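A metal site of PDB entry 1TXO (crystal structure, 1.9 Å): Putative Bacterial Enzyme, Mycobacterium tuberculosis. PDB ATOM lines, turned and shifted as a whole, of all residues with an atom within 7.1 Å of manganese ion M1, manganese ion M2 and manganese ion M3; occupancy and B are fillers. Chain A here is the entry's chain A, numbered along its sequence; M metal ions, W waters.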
ATOM      1  N   ARG A  17      17.641  37.236 -30.247  1.00  0.00           N
ATOM      2  CA  ARG A  17      18.648  36.170 -30.376  1.00  0.00           C
ATOM      3  C   ARG A  17      19.669  36.430 -31.479  1.00  0.00           C
ATOM      4  O   ARG A  17      19.373  37.076 -32.465  1.00  0.00           O
ATOM      5  CB  ARG A  17      17.979  34.802 -30.630  1.00  0.00           C
ATOM      6  CG  ARG A  17      16.955  34.362 -29.593  1.00  0.00           C
ATOM      7  CD  ARG A  17      17.379  34.546 -28.137  1.00  0.00           C
ATOM      8  NE  ARG A  17      16.275  34.266 -27.225  1.00  0.00           N
ATOM      9  CZ  ARG A  17      15.876  33.038 -26.875  1.00  0.00           C
ATOM     10  NH1 ARG A  17      16.477  31.966 -27.363  1.00  0.00           N
ATOM     11  NH2 ARG A  17      14.855  32.905 -26.040  1.00  0.00           N
ATOM     12  N   ASN A  20      19.323  31.578 -35.362  1.00  0.00           N
ATOM     13  CA  ASN A  20      18.057  30.863 -35.418  1.00  0.00           C
ATOM     14  C   ASN A  20      18.267  29.353 -35.248  1.00  0.00           C
ATOM     15  O   ASN A  20      18.777  28.687 -36.154  1.00  0.00           O
ATOM     16  CB  ASN A  20      17.314  31.158 -36.728  1.00  0.00           C
ATOM     17  CG  ASN A  20      15.865  30.684 -36.707  1.00  0.00           C
ATOM     18  OD1 ASN A  20      15.448  29.973 -35.780  1.00  0.00           O
ATOM     19  ND2 ASN A  20      15.105  31.070 -37.717  1.00  0.00           N
ATOM     20  N   GLU A  21      17.849  28.846 -34.090  1.00  0.00           N
ATOM     21  CA  GLU A  21      17.959  27.425 -33.755  1.00  0.00           C
ATOM     22  C   GLU A  21      16.654  26.623 -33.945  1.00  0.00           C
ATOM     23  O   GLU A  21      16.610  25.440 -33.617  1.00  0.00           O
ATOM     24  CB  GLU A  21      18.512  27.285 -32.333  1.00  0.00           C
ATOM     25  CG  GLU A  21      19.934  27.818 -32.249  1.00  0.00           C
ATOM     26  CD  GLU A  21      20.466  28.044 -30.852  1.00  0.00           C
ATOM     27  OE1 GLU A  21      19.857  27.571 -29.868  1.00  0.00           O
ATOM     28  OE2 GLU A  21      21.533  28.689 -30.749  1.00  0.00           O
ATOM     29  N   ASP A  22      15.604  27.248 -34.476  1.00  0.00           N
ATOM     30  CA  ASP A  22      14.438  26.514 -34.963  1.00  0.00           C
ATOM     31  C   ASP A  22      14.756  25.884 -36.333  1.00  0.00           C
ATOM     32  O   ASP A  22      15.446  26.468 -37.152  1.00  0.00           O
ATOM     33  CB  ASP A  22      13.232  27.435 -35.173  1.00  0.00           C
ATOM     34  CG  ASP A  22      12.613  27.937 -33.875  1.00  0.00           C
ATOM     35  OD1 ASP A  22      13.014  27.502 -32.766  1.00  0.00           O
ATOM     36  OD2 ASP A  22      11.698  28.789 -33.905  1.00  0.00           O
ATOM     37  N   ALA A  34      11.100  21.772 -35.064  1.00  0.00           N
ATOM     38  CA  ALA A  34      12.026  21.445 -33.993  1.00  0.00           C
ATOM     39  C   ALA A  34      12.657  22.711 -33.459  1.00  0.00           C
ATOM     40  O   ALA A  34      13.335  23.436 -34.203  1.00  0.00           O
ATOM     41  CB  ALA A  34      13.089  20.485 -34.499  1.00  0.00           C
ATOM     42  N   ASP A  35      12.425  23.007 -32.186  1.00  0.00           N
ATOM     43  CA  ASP A  35      12.982  24.180 -31.523  1.00  0.00           C
ATOM     44  C   ASP A  35      14.223  23.743 -30.746  1.00  0.00           C
ATOM     45  O   ASP A  35      14.130  23.115 -29.692  1.00  0.00           O
ATOM     46  CB  ASP A  35      11.939  24.808 -30.611  1.00  0.00           C
ATOM     47  CG  ASP A  35      12.478  25.986 -29.820  1.00  0.00           C
ATOM     48  OD1 ASP A  35      13.708  26.188 -29.794  1.00  0.00           O
ATOM     49  OD2 ASP A  35      11.742  26.748 -29.180  1.00  0.00           O
ATOM     50  N   GLY A  36      15.378  24.067 -31.309  1.00  0.00           N
ATOM     51  CA  GLY A  36      16.659  23.617 -30.780  1.00  0.00           C
ATOM     52  C   GLY A  36      17.188  24.487 -29.667  1.00  0.00           C
ATOM     53  O   GLY A  36      16.864  25.666 -29.569  1.00  0.00           O
ATOM     54  N   MET A  37      18.038  23.905 -28.832  1.00  0.00           N
ATOM     55  CA  MET A  37      18.712  24.639 -27.768  1.00  0.00           C
ATOM     56  C   MET A  37      20.143  24.134 -27.578  1.00  0.00           C
ATOM     57  O   MET A  37      20.439  22.967 -27.831  1.00  0.00           O
ATOM     58  CB  MET A  37      17.946  24.472 -26.460  1.00  0.00           C
ATOM     59  CG  MET A  37      18.020  23.060 -25.894  1.00  0.00           C
ATOM     60  SD  MET A  37      16.758  22.778 -24.431  1.00  0.00           S
ATOM     61  CE  MET A  37      16.317  20.944 -24.790  1.00  0.00           C
ATOM     62  N   GLY A  38      21.006  25.014 -27.108  1.00  0.00           N
ATOM     63  CA  GLY A  38      22.404  24.677 -26.883  1.00  0.00           C
ATOM     64  C   GLY A  38      23.322  25.828 -27.235  1.00  0.00           C
ATOM     65  O   GLY A  38      23.178  26.465 -28.277  1.00  0.00           O
ATOM     66  N   GLY A  43      22.204  24.425 -30.647  1.00  0.00           N
ATOM     67  CA  GLY A  43      20.793  24.243 -30.885  1.00  0.00           C
ATOM     68  C   GLY A  43      20.446  24.112 -32.360  1.00  0.00           C
ATOM     69  O   GLY A  43      19.496  23.434 -32.694  1.00  0.00           O
ATOM     70  N   GLY A  95      19.902  20.018 -27.332  1.00  0.00           N
ATOM     71  CA  GLY A  95      18.693  19.257 -27.559  1.00  0.00           C
ATOM     72  C   GLY A  95      17.663  20.029 -28.352  1.00  0.00           C
ATOM     73  O   GLY A  95      17.932  21.117 -28.819  1.00  0.00           O
ATOM     74  N   THR A  97      13.044  20.343 -29.131  1.00  0.00           N
ATOM     75  CA  THR A  97      11.677  19.877 -29.176  1.00  0.00           C
ATOM     76  C   THR A  97      11.461  19.243 -30.540  1.00  0.00           C
ATOM     77  O   THR A  97      12.277  19.389 -31.458  1.00  0.00           O
ATOM     78  CB  THR A  97      10.655  21.019 -29.022  1.00  0.00           C
ATOM     79  OG1 THR A  97      10.570  21.748 -30.247  1.00  0.00           O
ATOM     80  CG2 THR A  97      11.076  22.041 -27.981  1.00  0.00           C
ATOM     81  N   ASP A 115       7.928  21.983 -25.947  1.00  0.00           N
ATOM     82  CA  ASP A 115       6.985  23.087 -25.785  1.00  0.00           C
ATOM     83  C   ASP A 115       6.673  23.826 -27.092  1.00  0.00           C
ATOM     84  O   ASP A 115       6.071  24.905 -27.070  1.00  0.00           O
ATOM     85  CB  ASP A 115       7.423  24.052 -24.663  1.00  0.00           C
ATOM     86  CG  ASP A 115       8.677  24.839 -25.002  1.00  0.00           C
ATOM     87  OD1 ASP A 115       9.338  24.565 -26.039  1.00  0.00           O
ATOM     88  OD2 ASP A 115       9.082  25.783 -24.272  1.00  0.00           O
ATOM     89  N   SER A 116       7.090  23.250 -28.217  1.00  0.00           N
ATOM     90  CA  SER A 116       6.500  23.620 -29.501  1.00  0.00           C
ATOM     91  C   SER A 116       5.048  23.140 -29.468  1.00  0.00           C
ATOM     92  O   SER A 116       4.668  22.349 -28.597  1.00  0.00           O
ATOM     93  CB  SER A 116       7.269  23.032 -30.693  1.00  0.00           C
ATOM     94  OG  SER A 116       7.608  21.670 -30.491  1.00  0.00           O
ATOM     95  N   ASP A 132       1.962  20.751 -23.797  1.00  0.00           N
ATOM     96  CA  ASP A 132       3.231  21.413 -23.484  1.00  0.00           C
ATOM     97  C   ASP A 132       3.989  20.644 -22.416  1.00  0.00           C
ATOM     98  O   ASP A 132       3.400  20.258 -21.400  1.00  0.00           O
ATOM     99  CB  ASP A 132       2.975  22.810 -22.904  1.00  0.00           C
ATOM    100  CG  ASP A 132       2.741  23.861 -23.955  1.00  0.00           C
ATOM    101  OD1 ASP A 132       2.232  23.546 -25.060  1.00  0.00           O
ATOM    102  OD2 ASP A 132       3.027  25.061 -23.732  1.00  0.00           O
ATOM    103  N   ASP A 133       5.291  20.469 -22.634  1.00  0.00           N
ATOM    104  CA  ASP A 133       6.179  19.967 -21.603  1.00  0.00           C
ATOM    105  C   ASP A 133       6.855  21.175 -20.982  1.00  0.00           C
ATOM    106  O   ASP A 133       8.042  21.405 -21.170  1.00  0.00           O
ATOM    107  CB  ASP A 133       7.198  18.998 -22.197  1.00  0.00           C
ATOM    108  CG  ASP A 133       6.561  17.689 -22.616  1.00  0.00           C
ATOM    109  OD1 ASP A 133       5.690  17.194 -21.869  1.00  0.00           O
ATOM    110  OD2 ASP A 133       6.857  17.072 -23.662  1.00  0.00           O
ATOM    111  N   THR A 134       6.065  21.962 -20.245  1.00  0.00           N
ATOM    112  CA  THR A 134       6.577  23.137 -19.551  1.00  0.00           C
ATOM    113  C   THR A 134       6.370  22.980 -18.062  1.00  0.00           C
ATOM    114  O   THR A 134       5.606  22.135 -17.609  1.00  0.00           O
ATOM    115  CB  THR A 134       5.863  24.412 -20.000  1.00  0.00           C
ATOM    116  OG1 THR A 134       4.447  24.292 -19.778  1.00  0.00           O
ATOM    117  CG2 THR A 134       6.023  24.662 -21.510  1.00  0.00           C
ATOM    118  N   ARG A 156       6.921  30.175 -17.131  1.00  0.00           N
ATOM    119  CA  ARG A 156       5.863  29.624 -17.978  1.00  0.00           C
ATOM    120  C   ARG A 156       6.359  29.006 -19.299  1.00  0.00           C
ATOM    121  O   ARG A 156       5.725  28.096 -19.810  1.00  0.00           O
ATOM    122  CB  ARG A 156       4.771  30.674 -18.242  1.00  0.00           C
ATOM    123  CG  ARG A 156       5.203  31.914 -18.990  1.00  0.00           C
ATOM    124  CD  ARG A 156       4.072  32.898 -19.240  1.00  0.00           C
ATOM    125  NE  ARG A 156       4.554  34.179 -19.754  1.00  0.00           N
ATOM    126  CZ  ARG A 156       5.049  35.160 -19.007  1.00  0.00           C
ATOM    127  NH1 ARG A 156       5.140  35.045 -17.692  1.00  0.00           N
ATOM    128  NH2 ARG A 156       5.471  36.278 -19.592  1.00  0.00           N
ATOM    129  N   SER A 157       7.487  29.486 -19.822  1.00  0.00           N
ATOM    130  CA  SER A 157       8.075  28.923 -21.045  1.00  0.00           C
ATOM    131  C   SER A 157       9.103  27.811 -20.787  1.00  0.00           C
ATOM    132  O   SER A 157       9.615  27.208 -21.733  1.00  0.00           O
ATOM    133  CB  SER A 157       8.722  30.025 -21.891  1.00  0.00           C
ATOM    134  OG  SER A 157       9.158  29.517 -23.156  1.00  0.00           O
ATOM    135  N   LEU A 158       9.389  27.530 -19.516  1.00  0.00           N
ATOM    136  CA  LEU A 158      10.472  26.627 -19.164  1.00  0.00           C
ATOM    137  C   LEU A 158      10.191  25.206 -19.602  1.00  0.00           C
ATOM    138  O   LEU A 158       9.205  24.606 -19.210  1.00  0.00           O
ATOM    139  CB  LEU A 158      10.739  26.642 -17.652  1.00  0.00           C
ATOM    140  CG  LEU A 158      11.904  25.758 -17.223  1.00  0.00           C
ATOM    141  CD1 LEU A 158      13.218  26.274 -17.821  1.00  0.00           C
ATOM    142  CD2 LEU A 158      11.974  25.701 -15.706  1.00  0.00           C
ATOM    143  N   ILE A 159      11.085  24.659 -20.420  1.00  0.00           N
ATOM    144  CA  ILE A 159      10.886  23.343 -20.988  1.00  0.00           C
ATOM    145  C   ILE A 159      11.404  22.269 -20.025  1.00  0.00           C
ATOM    146  O   ILE A 159      12.447  22.439 -19.389  1.00  0.00           O
ATOM    147  CB  ILE A 159      11.523  23.256 -22.406  1.00  0.00           C
ATOM    148  CG1 ILE A 159      11.273  21.894 -23.034  1.00  0.00           C
ATOM    149  CG2 ILE A 159      13.002  23.655 -22.400  1.00  0.00           C
ATOM    150  CD1 ILE A 159      11.551  21.854 -24.507  1.00  0.00           C
ATOM    151  N   SER A 187       6.827  27.122 -32.945  1.00  0.00           N
ATOM    152  CA  SER A 187       7.726  27.141 -31.813  1.00  0.00           C
ATOM    153  C   SER A 187       7.132  28.082 -30.758  1.00  0.00           C
ATOM    154  O   SER A 187       6.236  28.876 -31.062  1.00  0.00           O
ATOM    155  CB  SER A 187       9.138  27.587 -32.211  1.00  0.00           C
ATOM    156  OG  SER A 187       9.192  28.960 -32.588  1.00  0.00           O
ATOM    157  N   ASP A 188       7.639  27.974 -29.533  1.00  0.00           N
ATOM    158  CA  ASP A 188       7.176  28.838 -28.445  1.00  0.00           C
ATOM    159  C   ASP A 188       7.473  30.317 -28.718  1.00  0.00           C
ATOM    160  O   ASP A 188       6.928  31.171 -28.034  1.00  0.00           O
ATOM    161  CB  ASP A 188       7.749  28.398 -27.087  1.00  0.00           C
ATOM    162  CG  ASP A 188       9.260  28.493 -27.015  1.00  0.00           C
ATOM    163  OD1 ASP A 188       9.937  28.735 -28.057  1.00  0.00           O
ATOM    164  OD2 ASP A 188       9.844  28.335 -25.926  1.00  0.00           O
ATOM    165  N   GLY A 189       8.302  30.618 -29.702  1.00  0.00           N
ATOM    166  CA  GLY A 189       8.503  31.984 -30.143  1.00  0.00           C
ATOM    167  C   GLY A 189       7.242  32.669 -30.647  1.00  0.00           C
ATOM    168  O   GLY A 189       7.182  33.896 -30.671  1.00  0.00           O
ATOM    169  N   LEU A 190       6.268  31.880 -31.082  1.00  0.00           N
ATOM    170  CA  LEU A 190       4.943  32.418 -31.408  1.00  0.00           C
ATOM    171  C   LEU A 190       4.035  32.497 -30.189  1.00  0.00           C
ATOM    172  O   LEU A 190       3.499  33.560 -29.876  1.00  0.00           O
ATOM    173  CB  LEU A 190       4.236  31.563 -32.483  1.00  0.00           C
ATOM    174  CG  LEU A 190       2.770  31.948 -32.758  1.00  0.00           C
ATOM    175  CD1 LEU A 190       2.685  33.392 -33.229  1.00  0.00           C
ATOM    176  CD2 LEU A 190       2.106  31.011 -33.766  1.00  0.00           C
ATOM    177  N   ASP A 192       4.409  32.086 -26.883  1.00  0.00           N
ATOM    178  CA  ASP A 192       4.791  32.799 -25.666  1.00  0.00           C
ATOM    179  C   ASP A 192       4.218  34.254 -25.725  1.00  0.00           C
ATOM    180  O   ASP A 192       3.459  34.648 -24.829  1.00  0.00           O
ATOM    181  CB  ASP A 192       6.310  32.778 -25.416  1.00  0.00           C
ATOM    182  CG  ASP A 192       6.827  31.424 -24.876  1.00  0.00           C
ATOM    183  OD1 ASP A 192       6.017  30.513 -24.556  1.00  0.00           O
ATOM    184  OD2 ASP A 192       8.057  31.185 -24.739  1.00  0.00           O
ATOM    185  N   ASP A 226      12.291  35.644 -29.034  1.00  0.00           N
ATOM    186  CA  ASP A 226      12.839  34.335 -29.386  1.00  0.00           C
ATOM    187  C   ASP A 226      12.761  34.117 -30.913  1.00  0.00           C
ATOM    188  O   ASP A 226      12.075  34.852 -31.625  1.00  0.00           O
ATOM    189  CB  ASP A 226      12.000  33.270 -28.649  1.00  0.00           C
ATOM    190  CG  ASP A 226      12.627  31.880 -28.667  1.00  0.00           C
ATOM    191  OD1 ASP A 226      13.806  31.693 -29.034  1.00  0.00           O
ATOM    192  OD2 ASP A 226      11.959  30.878 -28.302  1.00  0.00           O
ATOM    193  N   ASN A 227      13.505  33.116 -31.395  1.00  0.00           N
ATOM    194  CA  ASN A 227      13.242  32.544 -32.715  1.00  0.00           C
ATOM    195  C   ASN A 227      11.768  32.164 -32.832  1.00  0.00           C
ATOM    196  O   ASN A 227      11.207  31.596 -31.892  1.00  0.00           O
ATOM    197  CB  ASN A 227      14.084  31.277 -32.959  1.00  0.00           C
ATOM    198  CG  ASN A 227      15.566  31.475 -32.689  1.00  0.00           C
ATOM    199  OD1 ASN A 227      16.255  30.535 -32.273  1.00  0.00           O
ATOM    200  ND2 ASN A 227      16.082  32.685 -32.922  1.00  0.00           N
ATOM    201  N   VAL A 228      11.130  32.484 -33.950  1.00  0.00           N
ATOM    202  CA  VAL A 228       9.720  32.163 -34.152  1.00  0.00           C
ATOM    203  C   VAL A 228       9.548  31.463 -35.481  1.00  0.00           C
ATOM    204  O   VAL A 228       9.995  31.939 -36.518  1.00  0.00           O
ATOM    205  CB  VAL A 228       8.804  33.421 -34.051  1.00  0.00           C
ATOM    206  CG1 VAL A 228       9.260  34.536 -34.977  1.00  0.00           C
ATOM    207  CG2 VAL A 228       7.322  33.051 -34.310  1.00  0.00           C
HETATM  208 MN    MN M   1      12.024  28.812 -28.574  1.00  0.00          MN
HETATM  209 MN    MN M   2      15.439  27.353 -29.313  1.00  0.00          MN
HETATM  210 MN    MN M   3       9.422  27.588 -23.829  1.00  0.00          MN
HETATM  211  O   HOH W   1      11.652  29.232 -30.710  1.00  0.00           O
HETATM  212  O   HOH W   2      11.382  27.023 -23.769  1.00  0.00           O
HETATM  213  O   HOH W   3      12.393  28.288 -26.475  1.00  0.00           O
HETATM  214  O   HOH W   4      14.130  29.097 -28.530  1.00  0.00           O
HETATM  215  O   HOH W   5      15.280  28.294 -31.484  1.00  0.00           O
HETATM  216  O   HOH W   6       7.156  27.777 -23.837  1.00  0.00           O
HETATM  217  O   HOH W   7      15.001  26.747 -27.190  1.00  0.00           O
HETATM  218  O   HOH W   8      17.478  28.565 -28.846  1.00  0.00           O
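Residues that only touch manganese ion M3: Asp 192 (3.95 Å).
Of the 29 residues printed, 4 come within 4 Å of manganese ion M3.
The nearest printed residue that does not touch manganese ion M3 is Leu 158 (4.3 Å).
Water W1 lies within hydrogen-bond range of O of Asn 227, OD1 of Asp 22 and OG of Ser 187.
Water W5 lies within hydrogen-bond range of the side-chain amide oxygen of Asn 227 (2.6 Å) and the side-chain carboxylate of Asp 22 (2.7 Å).
Manganese ion M2 is bound by OD1 of Asp 35, O of Gly 36, water W7, water W4, water W5 and water W8.
Manganese ion M3 is bound by OD2 of Asp 115 (1.9 Å).
Manganese ion M3 is bound by water W2, 2.0 Å away.
Manganese ion M3 is bound by the side-chain hydroxyl (OG) of Ser 157, at 2.1 Å.
O of Ser 157 binds manganese ion M3 (2.1 Å).
OD2 of Asp 188 is bound to manganese ion M3 (2.3 Å).
Water W6 binds manganese ion M3, 2.3 Å away.
The side-chain carboxylate (OD2) of Asp 192 lies close to the side-chain hydroxyl (OG) of Ser 157, 2.5 Å away.
The side-chain carboxylate (OD1) of Asp 226 is in salt-bridge range of the guanidinium group (NH1) of Arg 17, 3.2 Å away.
OG1 of Thr 97 lies within hydrogen-bond range of N of Asp 35 (3.0 Å).
The backbone NH (N) of Gly 36 is in hydrogen-bond range of the backbone carbonyl oxygen (O) of Glu 21.
Three residues have an atom within 4 Å of manganese ion M1: Asp 35, Asp 188 and Asp 226.
The nearest printed residue that does not touch manganese ion M1 is Gly 189 (4.3 Å).
Manganese ion M1 is bound by the side-chain carboxylate (OD2) of Asp 226, water W4, the side-chain carboxylate (OD1) of Asp 188, the side-chain carboxylate (OD2) of Asp 35, water W3 and water W1.
Manganese ion M1 has six donor atoms within binding distance.
The nearest printed residue that does not touch manganese ion M2 is Asp 22 (4.2 Å).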
